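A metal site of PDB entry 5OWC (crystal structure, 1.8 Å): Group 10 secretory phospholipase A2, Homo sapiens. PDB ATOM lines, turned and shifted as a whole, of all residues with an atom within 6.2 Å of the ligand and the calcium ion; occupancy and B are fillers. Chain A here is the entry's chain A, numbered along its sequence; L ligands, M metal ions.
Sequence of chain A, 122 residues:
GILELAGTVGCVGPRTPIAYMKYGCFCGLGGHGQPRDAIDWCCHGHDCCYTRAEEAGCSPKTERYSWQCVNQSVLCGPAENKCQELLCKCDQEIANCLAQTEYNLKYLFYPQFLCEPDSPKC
N2 of the ligand is in hydrogen-bond range of O of Cys 43, at 3.5 Å.
N of Gly 28 lies close to O2 of the ligand (3.0 Å).
The backbone NH of Gly 30 lies within hydrogen-bond range of an oxygen (O1) of the ligand, 3.1 Å away.
ND1 of His 46 is in hydrogen-bond range of N2 of the ligand (3.0 Å).
The side-chain sulfur (SG) of Cys 43 forms a disulfide with the side-chain sulfur (SG) of Cys 27.
A fluorine (F1) of the ligand lies close to the backbone carbonyl oxygen of Pro 17, 3.3 Å away.
Leu 5 touches the ligand.
Ala 6 touches the ligand (CB to F3, 3.8 Å).
Ile 18 touches the ligand (CD1 to F3, 3.9 Å).
Tyr 20 touches the ligand.
Met 21 touches the ligand.
CA of Cys 27 touches O2 of the ligand, 3.7 Å away.
N of Leu 29 touches C10 of the ligand, at 3.5 Å.
Tyr 50 touches the ligand (CD2 to C18, 3.8 Å).
Ile 94 touches the ligand (CD1 to C5, 3.5 Å).
Hydrophobic or aromatic side chains that line the ligand: Leu 5, Ala 6, Pro 17, Ile 18, Tyr 20, Met 21, Leu 29, His 46, Tyr 50 and Ile 94.
Of the 25 residues printed, 16 come within 4 Å of the ligand.
The nearest printed residue that does not touch the ligand is Val 9 (4.1 Å).
The nearest printed residue that does not touch the calcium ion is Leu 29 (4.4 Å).
The calcium ion is bound by the backbone carbonyl oxygen (O) of Phe 26 (2.3 Å), an oxygen (O4) of the ligand (2.3 Å), the backbone carbonyl oxygen (O) of Gly 28 (2.3 Å), the backbone carbonyl oxygen (O) of Gly 30 (2.4 Å), an oxygen (O2) of the ligand (2.5 Å), the side-chain carboxylate (OD2) of Asp 47 (2.5 Å) and the side-chain carboxylate (OD1) of Asp 47 (2.5 Å).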
ATOM      1  N   ILE A   2       4.758  -9.161  28.178  1.00  0.00           N
ATOM      2  CA  ILE A   2       5.444 -10.361  28.693  1.00  0.00           C
ATOM      3  C   ILE A   2       4.646 -11.640  28.342  1.00  0.00           C
ATOM      4  O   ILE A   2       5.230 -12.679  28.083  1.00  0.00           O
ATOM      5  CB  ILE A   2       5.687 -10.258  30.223  1.00  0.00           C
ATOM      6  CG1 ILE A   2       6.894  -9.388  30.565  1.00  0.00           C
ATOM      7  CG2 ILE A   2       6.001 -11.611  30.848  1.00  0.00           C
ATOM      8  CD1 ILE A   2       7.626  -8.771  29.397  1.00  0.00           C
ATOM      9  N   LEU A   5       5.389 -12.424  24.787  1.00  0.00           N
ATOM     10  CA  LEU A   5       6.770 -12.860  24.713  1.00  0.00           C
ATOM     11  C   LEU A   5       6.915 -14.352  25.052  1.00  0.00           C
ATOM     12  O   LEU A   5       7.518 -15.127  24.294  1.00  0.00           O
ATOM     13  CB  LEU A   5       7.648 -12.008  25.639  1.00  0.00           C
ATOM     14  CG  LEU A   5       9.121 -12.424  25.752  1.00  0.00           C
ATOM     15  CD1 LEU A   5       9.811 -12.504  24.396  1.00  0.00           C
ATOM     16  CD2 LEU A   5       9.811 -11.405  26.649  1.00  0.00           C
ATOM     17  N   ALA A   6       6.353 -14.738  26.197  1.00  0.00           N
ATOM     18  CA  ALA A   6       6.365 -16.140  26.616  1.00  0.00           C
ATOM     19  C   ALA A   6       5.657 -17.032  25.573  1.00  0.00           C
ATOM     20  O   ALA A   6       6.169 -18.087  25.199  1.00  0.00           O
ATOM     21  CB  ALA A   6       5.696 -16.304  27.980  1.00  0.00           C
ATOM     22  N   VAL A   9       7.686 -17.223  22.119  1.00  0.00           N
ATOM     23  CA  VAL A   9       8.860 -18.055  22.353  1.00  0.00           C
ATOM     24  C   VAL A   9       8.461 -19.541  22.477  1.00  0.00           C
ATOM     25  O   VAL A   9       9.111 -20.409  21.890  1.00  0.00           O
ATOM     26  CB  VAL A   9       9.699 -17.535  23.541  1.00  0.00           C
ATOM     27  CG1 VAL A   9      10.803 -18.528  23.932  1.00  0.00           C
ATOM     28  CG2 VAL A   9      10.341 -16.200  23.197  1.00  0.00           C
ATOM     29  N   PRO A  17       9.432 -21.340  27.859  1.00  0.00           N
ATOM     30  CA  PRO A  17       9.950 -19.967  27.909  1.00  0.00           C
ATOM     31  C   PRO A  17      10.678 -19.619  29.225  1.00  0.00           C
ATOM     32  O   PRO A  17      11.549 -18.740  29.241  1.00  0.00           O
ATOM     33  CB  PRO A  17       8.704 -19.088  27.726  1.00  0.00           C
ATOM     34  CG  PRO A  17       7.539 -19.976  27.988  1.00  0.00           C
ATOM     35  CD  PRO A  17       7.977 -21.362  27.613  1.00  0.00           C
ATOM     36  N   ILE A  18      10.310 -20.343  30.290  1.00  0.00           N
ATOM     37  CA  ILE A  18      10.994 -20.340  31.602  1.00  0.00           C
ATOM     38  C   ILE A  18      12.506 -20.590  31.516  1.00  0.00           C
ATOM     39  O   ILE A  18      13.259 -20.095  32.345  1.00  0.00           O
ATOM     40  CB  ILE A  18      10.350 -21.402  32.555  1.00  0.00           C
ATOM     41  CG1 ILE A  18       8.867 -21.074  32.809  1.00  0.00           C
ATOM     42  CG2 ILE A  18      11.079 -21.501  33.895  1.00  0.00           C
ATOM     43  CD1 ILE A  18       8.585 -19.621  33.111  1.00  0.00           C
ATOM     44  N   ALA A  19      12.934 -21.344  30.501  1.00  0.00           N
ATOM     45  CA  ALA A  19      14.353 -21.605  30.258  1.00  0.00           C
ATOM     46  C   ALA A  19      15.181 -20.340  30.007  1.00  0.00           C
ATOM     47  O   ALA A  19      16.416 -20.384  30.100  1.00  0.00           O
ATOM     48  CB  ALA A  19      14.506 -22.550  29.095  1.00  0.00           C
ATOM     49  N   TYR A  20      14.523 -19.234  29.663  1.00  0.00           N
ATOM     50  CA  TYR A  20      15.200 -17.948  29.419  1.00  0.00           C
ATOM     51  C   TYR A  20      14.978 -16.862  30.476  1.00  0.00           C
ATOM     52  O   TYR A  20      15.362 -15.714  30.255  1.00  0.00           O
ATOM     53  CB  TYR A  20      14.750 -17.419  28.061  1.00  0.00           C
ATOM     54  CG  TYR A  20      14.829 -18.450  26.973  1.00  0.00           C
ATOM     55  CD1 TYR A  20      16.061 -18.878  26.490  1.00  0.00           C
ATOM     56  CD2 TYR A  20      13.674 -19.017  26.429  1.00  0.00           C
ATOM     57  CE1 TYR A  20      16.148 -19.828  25.492  1.00  0.00           C
ATOM     58  CE2 TYR A  20      13.751 -19.981  25.429  1.00  0.00           C
ATOM     59  CZ  TYR A  20      14.992 -20.375  24.958  1.00  0.00           C
ATOM     60  OH  TYR A  20      15.097 -21.308  23.947  1.00  0.00           O
ATOM     61  N   MET A  21      14.374 -17.206  31.614  1.00  0.00           N
ATOM     62  CA  MET A  21      14.036 -16.214  32.639  1.00  0.00           C
ATOM     63  C   MET A  21      15.250 -15.581  33.297  1.00  0.00           C
ATOM     64  O   MET A  21      15.241 -14.400  33.633  1.00  0.00           O
ATOM     65  CB  MET A  21      13.153 -16.827  33.724  1.00  0.00           C
ATOM     66  CG  MET A  21      11.684 -16.824  33.346  1.00  0.00           C
ATOM     67  SD  MET A  21      10.594 -17.432  34.638  1.00  0.00           S
ATOM     68  CE  MET A  21      10.248 -15.904  35.509  1.00  0.00           C
ATOM     69  N   CYS A  25      23.995 -13.513  30.508  1.00  0.00           N
ATOM     70  CA  CYS A  25      24.079 -12.126  30.942  1.00  0.00           C
ATOM     71  C   CYS A  25      22.890 -11.262  30.520  1.00  0.00           C
ATOM     72  O   CYS A  25      22.681 -10.201  31.095  1.00  0.00           O
ATOM     73  CB  CYS A  25      25.373 -11.525  30.423  1.00  0.00           C
ATOM     74  SG  CYS A  25      26.880 -12.190  31.200  1.00  0.00           S
ATOM     75  N   PHE A  26      22.103 -11.723  29.540  1.00  0.00           N
ATOM     76  CA  PHE A  26      21.033 -10.895  28.960  1.00  0.00           C
ATOM     77  C   PHE A  26      19.617 -11.421  29.057  1.00  0.00           C
ATOM     78  O   PHE A  26      18.678 -10.622  29.027  1.00  0.00           O
ATOM     79  CB  PHE A  26      21.371 -10.543  27.522  1.00  0.00           C
ATOM     80  CG  PHE A  26      22.506  -9.577  27.415  1.00  0.00           C
ATOM     81  CD1 PHE A  26      22.275  -8.214  27.561  1.00  0.00           C
ATOM     82  CD2 PHE A  26      23.805 -10.018  27.243  1.00  0.00           C
ATOM     83  CE1 PHE A  26      23.323  -7.301  27.491  1.00  0.00           C
ATOM     84  CE2 PHE A  26      24.853  -9.127  27.178  1.00  0.00           C
ATOM     85  CZ  PHE A  26      24.612  -7.762  27.310  1.00  0.00           C
ATOM     86  N   CYS A  27      19.430 -12.739  29.170  1.00  0.00           N
ATOM     87  CA  CYS A  27      18.085 -13.298  29.218  1.00  0.00           C
ATOM     88  C   CYS A  27      17.522 -13.154  30.616  1.00  0.00           C
ATOM     89  O   CYS A  27      17.990 -13.815  31.548  1.00  0.00           O
ATOM     90  CB  CYS A  27      18.054 -14.760  28.780  1.00  0.00           C
ATOM     91  SG  CYS A  27      18.814 -15.125  27.189  1.00  0.00           S
ATOM     92  N   GLY A  28      16.523 -12.287  30.747  1.00  0.00           N
ATOM     93  CA  GLY A  28      15.976 -11.863  32.034  1.00  0.00           C
ATOM     94  C   GLY A  28      15.907 -10.350  32.082  1.00  0.00           C
ATOM     95  O   GLY A  28      16.339  -9.672  31.152  1.00  0.00           O
ATOM     96  N   LEU A  29      15.392  -9.827  33.181  1.00  0.00           N
ATOM     97  CA  LEU A  29      15.227  -8.370  33.346  1.00  0.00           C
ATOM     98  C   LEU A  29      16.586  -7.671  33.317  1.00  0.00           C
ATOM     99  O   LEU A  29      17.497  -8.015  34.068  1.00  0.00           O
ATOM    100  CB  LEU A  29      14.485  -8.063  34.642  1.00  0.00           C
ATOM    101  CG  LEU A  29      14.043  -6.624  34.889  1.00  0.00           C
ATOM    102  CD1 LEU A  29      13.030  -6.143  33.845  1.00  0.00           C
ATOM    103  CD2 LEU A  29      13.442  -6.510  36.284  1.00  0.00           C
ATOM    104  N   GLY A  30      16.694  -6.683  32.424  1.00  0.00           N
ATOM    105  CA  GLY A  30      17.959  -5.996  32.153  1.00  0.00           C
ATOM    106  C   GLY A  30      19.000  -6.883  31.511  1.00  0.00           C
ATOM    107  O   GLY A  30      18.680  -7.830  30.780  1.00  0.00           O
ATOM    108  N   GLY A  31      20.252  -6.578  31.766  1.00  0.00           N
ATOM    109  CA  GLY A  31      21.349  -7.345  31.211  1.00  0.00           C
ATOM    110  C   GLY A  31      22.503  -6.468  30.819  1.00  0.00           C
ATOM    111  O   GLY A  31      22.322  -5.366  30.299  1.00  0.00           O
ATOM    112  N   CYS A  42      20.770 -13.631  21.236  1.00  0.00           N
ATOM    113  CA  CYS A  42      19.344 -13.436  20.927  1.00  0.00           C
ATOM    114  C   CYS A  42      18.709 -12.514  21.949  1.00  0.00           C
ATOM    115  O   CYS A  42      17.950 -11.625  21.592  1.00  0.00           O
ATOM    116  CB  CYS A  42      18.564 -14.756  20.919  1.00  0.00           C
ATOM    117  SG  CYS A  42      19.039 -15.984  19.687  1.00  0.00           S
ATOM    118  N   CYS A  43      19.003 -12.739  23.239  1.00  0.00           N
ATOM    119  CA  CYS A  43      18.422 -11.911  24.283  1.00  0.00           C
ATOM    120  C   CYS A  43      18.976 -10.480  24.240  1.00  0.00           C
ATOM    121  O   CYS A  43      18.235  -9.528  24.462  1.00  0.00           O
ATOM    122  CB  CYS A  43      18.627 -12.545  25.654  1.00  0.00           C
ATOM    123  SG  CYS A  43      17.679 -14.060  25.865  1.00  0.00           S
ATOM    124  N   HIS A  44      20.266 -10.337  23.929  1.00  0.00           N
ATOM    125  CA  HIS A  44      20.842  -9.003  23.772  1.00  0.00           C
ATOM    126  C   HIS A  44      20.106  -8.243  22.661  1.00  0.00           C
ATOM    127  O   HIS A  44      19.715  -7.085  22.846  1.00  0.00           O
ATOM    128  CB  HIS A  44      22.332  -9.101  23.458  1.00  0.00           C
ATOM    129  CG  HIS A  44      22.956  -7.775  23.120  1.00  0.00           C
ATOM    130  ND1 HIS A  44      23.072  -7.325  21.831  1.00  0.00           N
ATOM    131  CD2 HIS A  44      23.486  -6.812  23.906  1.00  0.00           C
ATOM    132  CE1 HIS A  44      23.648  -6.135  21.832  1.00  0.00           C
ATOM    133  NE2 HIS A  44      23.905  -5.791  23.081  1.00  0.00           N
ATOM    134  N   HIS A  46      17.116  -8.765  21.525  1.00  0.00           N
ATOM    135  CA  HIS A  46      15.771  -8.504  21.994  1.00  0.00           C
ATOM    136  C   HIS A  46      15.694  -7.323  22.982  1.00  0.00           C
ATOM    137  O   HIS A  46      14.802  -6.484  22.885  1.00  0.00           O
ATOM    138  CB  HIS A  46      15.190  -9.786  22.601  1.00  0.00           C
ATOM    139  CG  HIS A  46      13.720  -9.722  22.853  1.00  0.00           C
ATOM    140  ND1 HIS A  46      13.184  -9.765  24.117  1.00  0.00           N
ATOM    141  CD2 HIS A  46      12.679  -9.626  21.999  1.00  0.00           C
ATOM    142  CE1 HIS A  46      11.868  -9.705  24.036  1.00  0.00           C
ATOM    143  NE2 HIS A  46      11.530  -9.611  22.758  1.00  0.00           N
ATOM    144  N   ASP A  47      16.639  -7.257  23.925  1.00  0.00           N
ATOM    145  CA  ASP A  47      16.761  -6.098  24.819  1.00  0.00           C
ATOM    146  C   ASP A  47      16.897  -4.788  24.034  1.00  0.00           C
ATOM    147  O   ASP A  47      16.246  -3.791  24.361  1.00  0.00           O
ATOM    148  CB  ASP A  47      17.976  -6.240  25.748  1.00  0.00           C
ATOM    149  CG  ASP A  47      17.784  -7.311  26.803  1.00  0.00           C
ATOM    150  OD1 ASP A  47      16.767  -8.045  26.826  1.00  0.00           O
ATOM    151  OD2 ASP A  47      18.686  -7.429  27.672  1.00  0.00           O
ATOM    152  N   TYR A  50      13.455  -3.967  22.405  1.00  0.00           N
ATOM    153  CA  TYR A  50      12.584  -3.354  23.418  1.00  0.00           C
ATOM    154  C   TYR A  50      12.994  -1.921  23.772  1.00  0.00           C
ATOM    155  O   TYR A  50      12.117  -1.056  23.957  1.00  0.00           O
ATOM    156  CB  TYR A  50      12.537  -4.220  24.684  1.00  0.00           C
ATOM    157  CG  TYR A  50      11.487  -5.336  24.669  1.00  0.00           C
ATOM    158  CD1 TYR A  50      10.959  -5.856  23.474  1.00  0.00           C
ATOM    159  CD2 TYR A  50      11.023  -5.875  25.869  1.00  0.00           C
ATOM    160  CE1 TYR A  50       9.994  -6.858  23.486  1.00  0.00           C
ATOM    161  CE2 TYR A  50      10.069  -6.892  25.893  1.00  0.00           C
ATOM    162  CZ  TYR A  50       9.559  -7.375  24.696  1.00  0.00           C
ATOM    163  OH  TYR A  50       8.615  -8.392  24.720  1.00  0.00           O
ATOM    164  N   LYS A  61       6.701  -4.312  27.899  1.00  0.00           N
ATOM    165  CA  LYS A  61       6.375  -5.282  28.950  1.00  0.00           C
ATOM    166  C   LYS A  61       4.888  -5.515  29.175  1.00  0.00           C
ATOM    167  O   LYS A  61       4.495  -6.583  29.636  1.00  0.00           O
ATOM    168  CB  LYS A  61       7.061  -4.901  30.265  1.00  0.00           C
ATOM    169  CG  LYS A  61       8.579  -4.846  30.150  1.00  0.00           C
ATOM    170  CD  LYS A  61       9.290  -4.776  31.499  1.00  0.00           C
ATOM    171  CE  LYS A  61       9.553  -3.341  31.950  1.00  0.00           C
ATOM    172  NZ  LYS A  61      10.225  -3.285  33.284  1.00  0.00           N
ATOM    173  N   ILE A  94      12.966 -12.687  18.388  1.00  0.00           N
ATOM    174  CA  ILE A  94      13.641 -13.462  19.434  1.00  0.00           C
ATOM    175  C   ILE A  94      13.168 -14.917  19.422  1.00  0.00           C
ATOM    176  O   ILE A  94      13.984 -15.820  19.590  1.00  0.00           O
ATOM    177  CB  ILE A  94      13.579 -12.857  20.856  1.00  0.00           C
ATOM    178  CG1 ILE A  94      14.742 -13.439  21.703  1.00  0.00           C
ATOM    179  CG2 ILE A  94      12.196 -13.013  21.489  1.00  0.00           C
ATOM    180  CD1 ILE A  94      14.641 -13.254  23.202  1.00  0.00           C
ATOM    181  N   LEU A  98      15.863 -17.903  19.075  1.00  0.00           N
ATOM    182  CA  LEU A  98      16.049 -18.920  20.122  1.00  0.00           C
ATOM    183  C   LEU A  98      15.766 -20.338  19.645  1.00  0.00           C
ATOM    184  O   LEU A  98      16.398 -21.281  20.091  1.00  0.00           O
ATOM    185  CB  LEU A  98      15.185 -18.599  21.330  1.00  0.00           C
ATOM    186  CG  LEU A  98      15.559 -17.307  22.065  1.00  0.00           C
ATOM    187  CD1 LEU A  98      14.470 -16.960  23.076  1.00  0.00           C
ATOM    188  CD2 LEU A  98      16.908 -17.417  22.760  1.00  0.00           C
HETATM  189  C1  LIG L   1      12.517 -15.174  26.543  1.00  0.00           C
HETATM  190  C2  LIG L   1      11.454 -15.770  27.150  1.00  0.00           C
HETATM  191  C3  LIG L   1      10.867 -15.190  28.281  1.00  0.00           C
HETATM  192  C4  LIG L   1      14.131 -12.064  27.444  1.00  0.00           C
HETATM  193  C5  LIG L   1      14.095 -13.135  26.610  1.00  0.00           C
HETATM  194  C6  LIG L   1      15.100 -10.960  27.367  1.00  0.00           C
HETATM  195  C7  LIG L   1      12.848 -11.261  29.423  1.00  0.00           C
HETATM  196  C8  LIG L   1       9.473 -15.729  30.154  1.00  0.00           C
HETATM  197  C9  LIG L   1      12.685 -11.552  30.779  1.00  0.00           C
HETATM  198  C10 LIG L   1      12.364 -10.534  31.671  1.00  0.00           C
HETATM  199  C11 LIG L   1      12.185  -9.227  31.222  1.00  0.00           C
HETATM  200  C12 LIG L   1      12.347  -8.923  29.868  1.00  0.00           C
HETATM  201  C13 LIG L   1      12.162  -7.521  29.347  1.00  0.00           C
HETATM  202  O1  LIG L   1      14.284  -5.942  30.572  1.00  0.00           O
HETATM  203  C14 LIG L   1      11.350 -13.983  28.794  1.00  0.00           C
HETATM  204  C15 LIG L   1      13.030 -13.964  27.042  1.00  0.00           C
HETATM  205  C16 LIG L   1      12.452 -13.355  28.177  1.00  0.00           C
HETATM  206  N1  LIG L   1      13.154 -12.209  28.426  1.00  0.00           N
HETATM  207  N2  LIG L   1      15.331 -10.368  26.173  1.00  0.00           N
HETATM  208  O2  LIG L   1      15.701 -10.583  28.384  1.00  0.00           O
HETATM  209  O3  LIG L   1       9.795 -15.845  28.794  1.00  0.00           O
HETATM  210  F1  LIG L   1      10.651 -16.023  30.834  1.00  0.00           F
HETATM  211  F2  LIG L   1       8.997 -14.435  30.410  1.00  0.00           F
HETATM  212  F3  LIG L   1       8.512 -16.687  30.472  1.00  0.00           F
HETATM  213  C17 LIG L   1      12.649  -9.950  28.982  1.00  0.00           C
HETATM  214  C18 LIG L   1      13.406  -6.979  28.621  1.00  0.00           C
HETATM  215  C19 LIG L   1      14.509  -6.633  29.606  1.00  0.00           C
HETATM  216  O4  LIG L   1      15.757  -7.068  29.429  1.00  0.00           O
HETATM  217 CA    CA M   1      17.256  -8.837  29.160  1.00  0.00          CA
